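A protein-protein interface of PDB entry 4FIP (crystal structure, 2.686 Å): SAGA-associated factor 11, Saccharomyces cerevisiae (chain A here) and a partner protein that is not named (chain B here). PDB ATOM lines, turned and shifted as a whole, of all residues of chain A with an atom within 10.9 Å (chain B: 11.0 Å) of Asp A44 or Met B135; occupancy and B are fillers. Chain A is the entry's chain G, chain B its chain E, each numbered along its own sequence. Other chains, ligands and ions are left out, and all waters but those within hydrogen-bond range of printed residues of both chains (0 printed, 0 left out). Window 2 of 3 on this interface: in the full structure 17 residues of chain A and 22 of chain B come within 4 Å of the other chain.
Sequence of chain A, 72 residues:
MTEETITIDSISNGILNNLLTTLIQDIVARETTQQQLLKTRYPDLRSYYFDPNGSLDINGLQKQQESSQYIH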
ATOM      1  N   GLN A  35      16.582 -21.103  27.203  1.00  0.00           N
ATOM      2  CA  GLN A  35      17.753 -21.013  26.326  1.00  0.00           C
ATOM      3  C   GLN A  35      18.018 -22.330  25.645  1.00  0.00           C
ATOM      4  O   GLN A  35      18.271 -22.367  24.455  1.00  0.00           O
ATOM      5  CB  GLN A  35      19.026 -20.609  27.090  1.00  0.00           C
ATOM      6  CG  GLN A  35      19.525 -19.182  26.880  1.00  0.00           C
ATOM      7  CD  GLN A  35      19.555 -18.726  25.425  1.00  0.00           C
ATOM      8  OE1 GLN A  35      18.522 -18.373  24.847  1.00  0.00           O
ATOM      9  NE2 GLN A  35      20.744 -18.683  24.846  1.00  0.00           N
ATOM     10  N   LEU A  37      15.869 -24.704  24.995  1.00  0.00           N
ATOM     11  CA  LEU A  37      14.841 -24.997  24.013  1.00  0.00           C
ATOM     12  C   LEU A  37      15.070 -24.179  22.759  1.00  0.00           C
ATOM     13  O   LEU A  37      14.897 -24.696  21.651  1.00  0.00           O
ATOM     14  CB  LEU A  37      13.450 -24.686  24.556  1.00  0.00           C
ATOM     15  CG  LEU A  37      12.304 -24.695  23.524  1.00  0.00           C
ATOM     16  CD1 LEU A  37      12.289 -26.000  22.747  1.00  0.00           C
ATOM     17  CD2 LEU A  37      10.961 -24.469  24.204  1.00  0.00           C
ATOM     18  N   LEU A  38      15.418 -22.902  22.922  1.00  0.00           N
ATOM     19  CA  LEU A  38      15.698 -22.047  21.767  1.00  0.00           C
ATOM     20  C   LEU A  38      16.961 -22.514  21.040  1.00  0.00           C
ATOM     21  O   LEU A  38      16.973 -22.615  19.815  1.00  0.00           O
ATOM     22  CB  LEU A  38      15.815 -20.558  22.149  1.00  0.00           C
ATOM     23  CG  LEU A  38      14.536 -19.747  22.481  1.00  0.00           C
ATOM     24  CD1 LEU A  38      14.916 -18.328  22.888  1.00  0.00           C
ATOM     25  CD2 LEU A  38      13.525 -19.717  21.333  1.00  0.00           C
ATOM     26  N   LYS A  39      18.018 -22.813  21.788  1.00  0.00           N
ATOM     27  CA  LYS A  39      19.268 -23.243  21.169  1.00  0.00           C
ATOM     28  C   LYS A  39      19.128 -24.569  20.408  1.00  0.00           C
ATOM     29  O   LYS A  39      19.827 -24.746  19.435  1.00  0.00           O
ATOM     30  CB  LYS A  39      20.438 -23.310  22.183  1.00  0.00           C
ATOM     31  CG  LYS A  39      21.296 -22.032  22.303  1.00  0.00           C
ATOM     32  CD  LYS A  39      22.571 -22.283  23.136  1.00  0.00           C
ATOM     33  CE  LYS A  39      23.463 -21.047  23.358  1.00  0.00           C
ATOM     34  NZ  LYS A  39      24.755 -21.328  24.083  1.00  0.00           N
ATOM     35  N   THR A  40      18.244 -25.483  20.819  1.00  0.00           N
ATOM     36  CA  THR A  40      18.127 -26.764  20.103  1.00  0.00           C
ATOM     37  C   THR A  40      17.088 -26.656  18.982  1.00  0.00           C
ATOM     38  O   THR A  40      17.238 -27.261  17.922  1.00  0.00           O
ATOM     39  CB  THR A  40      17.870 -28.017  21.011  1.00  0.00           C
ATOM     40  OG1 THR A  40      16.526 -28.483  20.872  1.00  0.00           O
ATOM     41  CG2 THR A  40      18.181 -27.766  22.485  1.00  0.00           C
ATOM     42  N   ARG A  41      16.041 -25.882  19.201  1.00  0.00           N
ATOM     43  CA  ARG A  41      15.050 -25.606  18.148  1.00  0.00           C
ATOM     44  C   ARG A  41      15.549 -24.751  16.949  1.00  0.00           C
ATOM     45  O   ARG A  41      15.109 -24.950  15.815  1.00  0.00           O
ATOM     46  CB  ARG A  41      13.875 -24.881  18.774  1.00  0.00           C
ATOM     47  CG  ARG A  41      12.892 -24.360  17.763  1.00  0.00           C
ATOM     48  CD  ARG A  41      11.707 -23.771  18.467  1.00  0.00           C
ATOM     49  NE  ARG A  41      10.964 -24.748  19.250  1.00  0.00           N
ATOM     50  CZ  ARG A  41       9.857 -24.440  19.921  1.00  0.00           C
ATOM     51  NH1 ARG A  41       9.400 -23.204  19.898  1.00  0.00           N
ATOM     52  NH2 ARG A  41       9.198 -25.363  20.607  1.00  0.00           N
ATOM     53  N   TYR A  42      16.417 -23.778  17.218  1.00  0.00           N
ATOM     54  CA  TYR A  42      16.892 -22.816  16.216  1.00  0.00           C
ATOM     55  C   TYR A  42      18.397 -22.800  16.244  1.00  0.00           C
ATOM     56  O   TYR A  42      18.993 -21.968  16.917  1.00  0.00           O
ATOM     57  CB  TYR A  42      16.382 -21.388  16.518  1.00  0.00           C
ATOM     58  CG  TYR A  42      14.883 -21.240  16.503  1.00  0.00           C
ATOM     59  CD1 TYR A  42      14.133 -21.628  15.396  1.00  0.00           C
ATOM     60  CD2 TYR A  42      14.212 -20.716  17.600  1.00  0.00           C
ATOM     61  CE1 TYR A  42      12.763 -21.511  15.401  1.00  0.00           C
ATOM     62  CE2 TYR A  42      12.840 -20.592  17.608  1.00  0.00           C
ATOM     63  CZ  TYR A  42      12.131 -20.990  16.508  1.00  0.00           C
ATOM     64  OH  TYR A  42      10.785 -20.848  16.518  1.00  0.00           O
ATOM     65  N   PRO A  43      19.028 -23.731  15.525  1.00  0.00           N
ATOM     66  CA  PRO A  43      20.484 -23.852  15.591  1.00  0.00           C
ATOM     67  C   PRO A  43      21.238 -22.548  15.304  1.00  0.00           C
ATOM     68  O   PRO A  43      22.250 -22.276  15.958  1.00  0.00           O
ATOM     69  CB  PRO A  43      20.783 -24.887  14.515  1.00  0.00           C
ATOM     70  CG  PRO A  43      19.558 -25.726  14.463  1.00  0.00           C
ATOM     71  CD  PRO A  43      18.441 -24.744  14.629  1.00  0.00           C
ATOM     72  N   ASP A  44      20.744 -21.742  14.363  1.00  0.00           N
ATOM     73  CA  ASP A  44      21.463 -20.529  13.951  1.00  0.00           C
ATOM     74  C   ASP A  44      20.771 -19.220  14.378  1.00  0.00           C
ATOM     75  O   ASP A  44      20.352 -18.428  13.531  1.00  0.00           O
ATOM     76  CB  ASP A  44      21.717 -20.561  12.425  1.00  0.00           C
ATOM     77  CG  ASP A  44      22.990 -21.343  12.046  1.00  0.00           C
ATOM     78  OD1 ASP A  44      23.976 -21.328  12.822  1.00  0.00           O
ATOM     79  OD2 ASP A  44      23.007 -21.957  10.957  1.00  0.00           O
ATOM     80  N   LEU A  45      20.694 -18.988  15.693  1.00  0.00           N
ATOM     81  CA  LEU A  45      20.088 -17.763  16.263  1.00  0.00           C
ATOM     82  C   LEU A  45      20.877 -16.487  15.935  1.00  0.00           C
ATOM     83  O   LEU A  45      22.092 -16.424  16.129  1.00  0.00           O
ATOM     84  CB  LEU A  45      19.920 -17.890  17.789  1.00  0.00           C
ATOM     85  CG  LEU A  45      18.604 -18.478  18.315  1.00  0.00           C
ATOM     86  CD1 LEU A  45      18.745 -19.030  19.730  1.00  0.00           C
ATOM     87  CD2 LEU A  45      17.518 -17.417  18.249  1.00  0.00           C
ATOM     88  N   MET B   6      22.054 -28.536  20.203  1.00  0.00           N
ATOM     89  CA  MET B   6      22.518 -29.300  21.397  1.00  0.00           C
ATOM     90  C   MET B   6      21.926 -30.720  21.380  1.00  0.00           C
ATOM     91  O   MET B   6      21.257 -31.103  20.420  1.00  0.00           O
ATOM     92  CB  MET B   6      22.142 -28.539  22.689  1.00  0.00           C
ATOM     93  CG  MET B   6      22.568 -27.062  22.702  1.00  0.00           C
ATOM     94  SD  MET B   6      22.589 -26.210  24.309  1.00  0.00           S
ATOM     95  CE  MET B   6      24.282 -26.445  24.884  1.00  0.00           C
ATOM     96  N   MET B 131       3.776 -27.051  12.785  1.00  0.00           N
ATOM     97  CA  MET B 131       5.214 -26.888  13.005  1.00  0.00           C
ATOM     98  C   MET B 131       5.497 -25.893  14.120  1.00  0.00           C
ATOM     99  O   MET B 131       4.625 -25.100  14.477  1.00  0.00           O
ATOM    100  CB  MET B 131       5.899 -26.420  11.725  1.00  0.00           C
ATOM    101  CG  MET B 131       5.212 -25.260  11.031  1.00  0.00           C
ATOM    102  SD  MET B 131       5.825 -25.038   9.353  1.00  0.00           S
ATOM    103  CE  MET B 131       4.731 -23.755   8.713  1.00  0.00           C
ATOM    104  N   VAL B 132       6.705 -25.939  14.686  1.00  0.00           N
ATOM    105  CA  VAL B 132       7.092 -24.944  15.660  1.00  0.00           C
ATOM    106  C   VAL B 132       7.230 -23.664  14.901  1.00  0.00           C
ATOM    107  O   VAL B 132       7.471 -23.717  13.718  1.00  0.00           O
ATOM    108  CB  VAL B 132       8.430 -25.211  16.369  1.00  0.00           C
ATOM    109  CG1 VAL B 132       8.298 -26.439  17.239  1.00  0.00           C
ATOM    110  CG2 VAL B 132       9.590 -25.281  15.375  1.00  0.00           C
ATOM    111  N   PRO B 133       7.095 -22.520  15.591  1.00  0.00           N
ATOM    112  CA  PRO B 133       7.217 -21.210  14.982  1.00  0.00           C
ATOM    113  C   PRO B 133       8.537 -20.975  14.270  1.00  0.00           C
ATOM    114  O   PRO B 133       9.571 -21.499  14.669  1.00  0.00           O
ATOM    115  CB  PRO B 133       7.112 -20.251  16.183  1.00  0.00           C
ATOM    116  CG  PRO B 133       6.307 -21.009  17.196  1.00  0.00           C
ATOM    117  CD  PRO B 133       6.818 -22.410  17.042  1.00  0.00           C
ATOM    118  N   SER B 134       8.475 -20.165  13.227  1.00  0.00           N
ATOM    119  CA  SER B 134       9.669 -19.693  12.548  1.00  0.00           C
ATOM    120  C   SER B 134      10.608 -18.952  13.498  1.00  0.00           C
ATOM    121  O   SER B 134      10.191 -18.391  14.498  1.00  0.00           O
ATOM    122  CB  SER B 134       9.269 -18.797  11.394  1.00  0.00           C
ATOM    123  OG  SER B 134      10.394 -18.084  10.973  1.00  0.00           O
ATOM    124  N   MET B 135      11.893 -18.968  13.209  1.00  0.00           N
ATOM    125  CA  MET B 135      12.844 -18.262  14.068  1.00  0.00           C
ATOM    126  C   MET B 135      12.546 -16.752  14.113  1.00  0.00           C
ATOM    127  O   MET B 135      12.707 -16.119  15.152  1.00  0.00           O
ATOM    128  CB  MET B 135      14.286 -18.466  13.575  1.00  0.00           C
ATOM    129  CG  MET B 135      15.355 -17.741  14.393  1.00  0.00           C
ATOM    130  SD  MET B 135      17.032 -18.059  13.798  1.00  0.00           S
ATOM    131  CE  MET B 135      17.393 -16.526  12.927  1.00  0.00           C
ATOM    132  N   GLU B 136      12.129 -16.187  12.987  1.00  0.00           N
ATOM    133  CA  GLU B 136      11.998 -14.747  12.878  1.00  0.00           C
ATOM    134  C   GLU B 136      10.558 -14.278  13.092  1.00  0.00           C
ATOM    135  O   GLU B 136      10.305 -13.088  13.121  1.00  0.00           O
ATOM    136  CB  GLU B 136      12.584 -14.209  11.548  1.00  0.00           C
ATOM    137  CG  GLU B 136      12.394 -15.080  10.308  1.00  0.00           C
ATOM    138  CD  GLU B 136      13.404 -16.221  10.228  1.00  0.00           C
ATOM    139  OE1 GLU B 136      12.980 -17.410  10.176  1.00  0.00           O
ATOM    140  OE2 GLU B 136      14.631 -15.929  10.258  1.00  0.00           O
ATOM    141  N   ARG B 137       9.616 -15.199  13.261  1.00  0.00           N
ATOM    142  CA  ARG B 137       8.236 -14.825  13.583  1.00  0.00           C
ATOM    143  C   ARG B 137       7.876 -15.089  15.025  1.00  0.00           C
ATOM    144  O   ARG B 137       6.876 -14.608  15.485  1.00  0.00           O
ATOM    145  CB  ARG B 137       7.218 -15.571  12.707  1.00  0.00           C
ATOM    146  CG  ARG B 137       7.403 -15.444  11.201  1.00  0.00           C
ATOM    147  CD  ARG B 137       6.921 -14.146  10.623  1.00  0.00           C
ATOM    148  NE  ARG B 137       7.965 -13.128  10.522  1.00  0.00           N
ATOM    149  CZ  ARG B 137       8.054 -12.010  11.254  1.00  0.00           C
ATOM    150  NH1 ARG B 137       7.183 -11.698  12.213  1.00  0.00           N
ATOM    151  NH2 ARG B 137       9.050 -11.179  11.031  1.00  0.00           N
ATOM    152  N   ARG B 138       8.672 -15.848  15.746  1.00  0.00           N
ATOM    153  CA  ARG B 138       8.248 -16.352  17.056  1.00  0.00           C
ATOM    154  C   ARG B 138       7.816 -15.268  18.056  1.00  0.00           C
ATOM    155  O   ARG B 138       7.007 -15.550  18.960  1.00  0.00           O
ATOM    156  CB  ARG B 138       9.367 -17.178  17.667  1.00  0.00           C
ATOM    157  CG  ARG B 138      10.597 -16.379  18.058  1.00  0.00           C
ATOM    158  CD  ARG B 138      11.785 -17.297  18.272  1.00  0.00           C
ATOM    159  NE  ARG B 138      12.782 -16.713  19.179  1.00  0.00           N
ATOM    160  CZ  ARG B 138      13.857 -16.017  18.809  1.00  0.00           C
ATOM    161  NH1 ARG B 138      14.129 -15.782  17.523  1.00  0.00           N
ATOM    162  NH2 ARG B 138      14.674 -15.565  19.752  1.00  0.00           N
ATOM    163  N   ASP B 139       8.362 -14.049  17.910  1.00  0.00           N
ATOM    164  CA  ASP B 139       8.051 -12.926  18.808  1.00  0.00           C
ATOM    165  C   ASP B 139       7.202 -11.824  18.128  1.00  0.00           C
ATOM    166  O   ASP B 139       7.094 -10.706  18.627  1.00  0.00           O
ATOM    167  CB  ASP B 139       9.356 -12.312  19.319  1.00  0.00           C
ATOM    168  CG  ASP B 139      10.114 -13.215  20.276  1.00  0.00           C
ATOM    169  OD1 ASP B 139       9.499 -13.676  21.272  1.00  0.00           O
ATOM    170  OD2 ASP B 139      11.335 -13.425  20.055  1.00  0.00           O
ATOM    171  N   GLY B 140       6.642 -12.122  16.963  1.00  0.00           N
ATOM    172  CA  GLY B 140       5.815 -11.169  16.227  1.00  0.00           C
ATOM    173  C   GLY B 140       6.426  -9.872  15.756  1.00  0.00           C
ATOM    174  O   GLY B 140       5.692  -8.972  15.334  1.00  0.00           O
ATOM    175  N   LEU B 141       7.747  -9.752  15.789  1.00  0.00           N
ATOM    176  CA  LEU B 141       8.407  -8.472  15.420  1.00  0.00           C
ATOM    177  C   LEU B 141       8.307  -8.266  13.911  1.00  0.00           C
ATOM    178  O   LEU B 141       8.549  -9.192  13.160  1.00  0.00           O
ATOM    179  CB  LEU B 141       9.878  -8.456  15.837  1.00  0.00           C
ATOM    180  CG  LEU B 141      10.120  -8.910  17.285  1.00  0.00           C
ATOM    181  CD1 LEU B 141      11.595  -9.152  17.593  1.00  0.00           C
ATOM    182  CD2 LEU B 141       9.505  -7.855  18.180  1.00  0.00           C
ATOM    183  N   SER B 142       7.916  -7.053  13.503  1.00  0.00           N
ATOM    184  CA  SER B 142       7.722  -6.649  12.107  1.00  0.00           C
ATOM    185  C   SER B 142       7.342  -5.202  12.118  1.00  0.00           C
ATOM    186  O   SER B 142       6.589  -4.788  12.960  1.00  0.00           O
ATOM    187  CB  SER B 142       6.587  -7.446  11.435  1.00  0.00           C
ATOM    188  OG  SER B 142       6.088  -6.829  10.235  1.00  0.00           O
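O of Asp A44 lies close to SD of Met B135 (3.4 Å). The backbone carbonyl oxygen of Pro B133 lies close to the side-chain hydroxyl of Tyr A42, 2.3 Å away. O of Ser B134 lies within hydrogen-bond range of OH of Tyr A42, 3.2 Å away.
The side-chain hydroxyl (OG) of Ser B134 lies within hydrogen-bond range of the side-chain carboxylate (OE1) of Glu B136, at 2.8 Å. The guanidinium group of Arg B138 lies within salt-bridge range of the side-chain carboxylate of Asp B139 (3.7 Å). O of Met B135 is in hydrogen-bond range of NH1 of Arg B138 (2.8 Å).
Leu A38 touches Arg B138 (CD2 to NE, 3.8 Å). Val B132 touches Arg A41 (CG1 to NH2, 3.6 Å). Arg A41 touches Pro B133. Met B135 touches Tyr A42. CD of Arg B138 touches CE2 of Tyr A42 (3.5 Å). CA of Leu A45 touches SD of Met B135, 3.9 Å away. CD2 of Leu A45 touches NH2 of Arg B138, at 3.7 Å.
Printed residues of chain B within 4 Å of Leu A38: Arg B138 (3.8 Å). Printed residues of chain B within 4 Å of Arg A41: Val B132 and Pro B133. Of chain B, only Pro B133, Ser B134, Met B135 and Arg B138 come within 4 Å of Tyr A42. No residue of chain B comes within 4 Å of Pro A43. Printed residues of chain B within 4 Å of Asp A44: Met B135. Of the printed residues of chain B, Leu A45 touches Met B135 (3.9 Å) and Arg B138 (3.7 Å). Met B6 touches none of the printed residues of chain A. Of the printed residues of chain A, Val B132 touches Arg A41. Of the printed residues of chain A, Pro B133 touches Arg A41 (3.9 Å) and Tyr A42 (2.3 Å). Ser B134 touches just one residue of chain A: Tyr A42. Met B135 touches just these residues of chain A: Tyr A42 (3.5 Å), Asp A44 (3.4 Å) and Leu A45 (3.9 Å). No residue of chain A comes within 4 Å of Glu B136. Of the printed residues of chain A, Arg B138 touches Leu A38, Tyr A42 and Leu A45. Asp B139 touches none of the printed residues of chain A. The nearest residue of chain B that does not touch Asp A44 is Glu B136 (7.0 Å). The nearest residue of chain A that does not touch Met B135 is Pro A43 (6.3 Å). The nearest printed residue of chain B that does not touch Arg A41 is Arg B138 (6.4 Å).
Of the 10 printed residues of chain A, 5 touch a printed residue of chain B. Hydrophobic or aromatic side chains of chain A within 4 Å of the printed part of chain B: Leu A38, Tyr A42 and Leu A45. Of the 13 printed residues of chain B, 5 touch a printed residue of chain A. Hydrophobic or aromatic side chains of chain B within 4 Å of the printed part of chain A: Val B132, Pro B133 and Met B135. Among the printed residues, no Asp or Glu carboxylate lies within 4 Å of a Lys or Arg side-chain nitrogen of the other chain.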
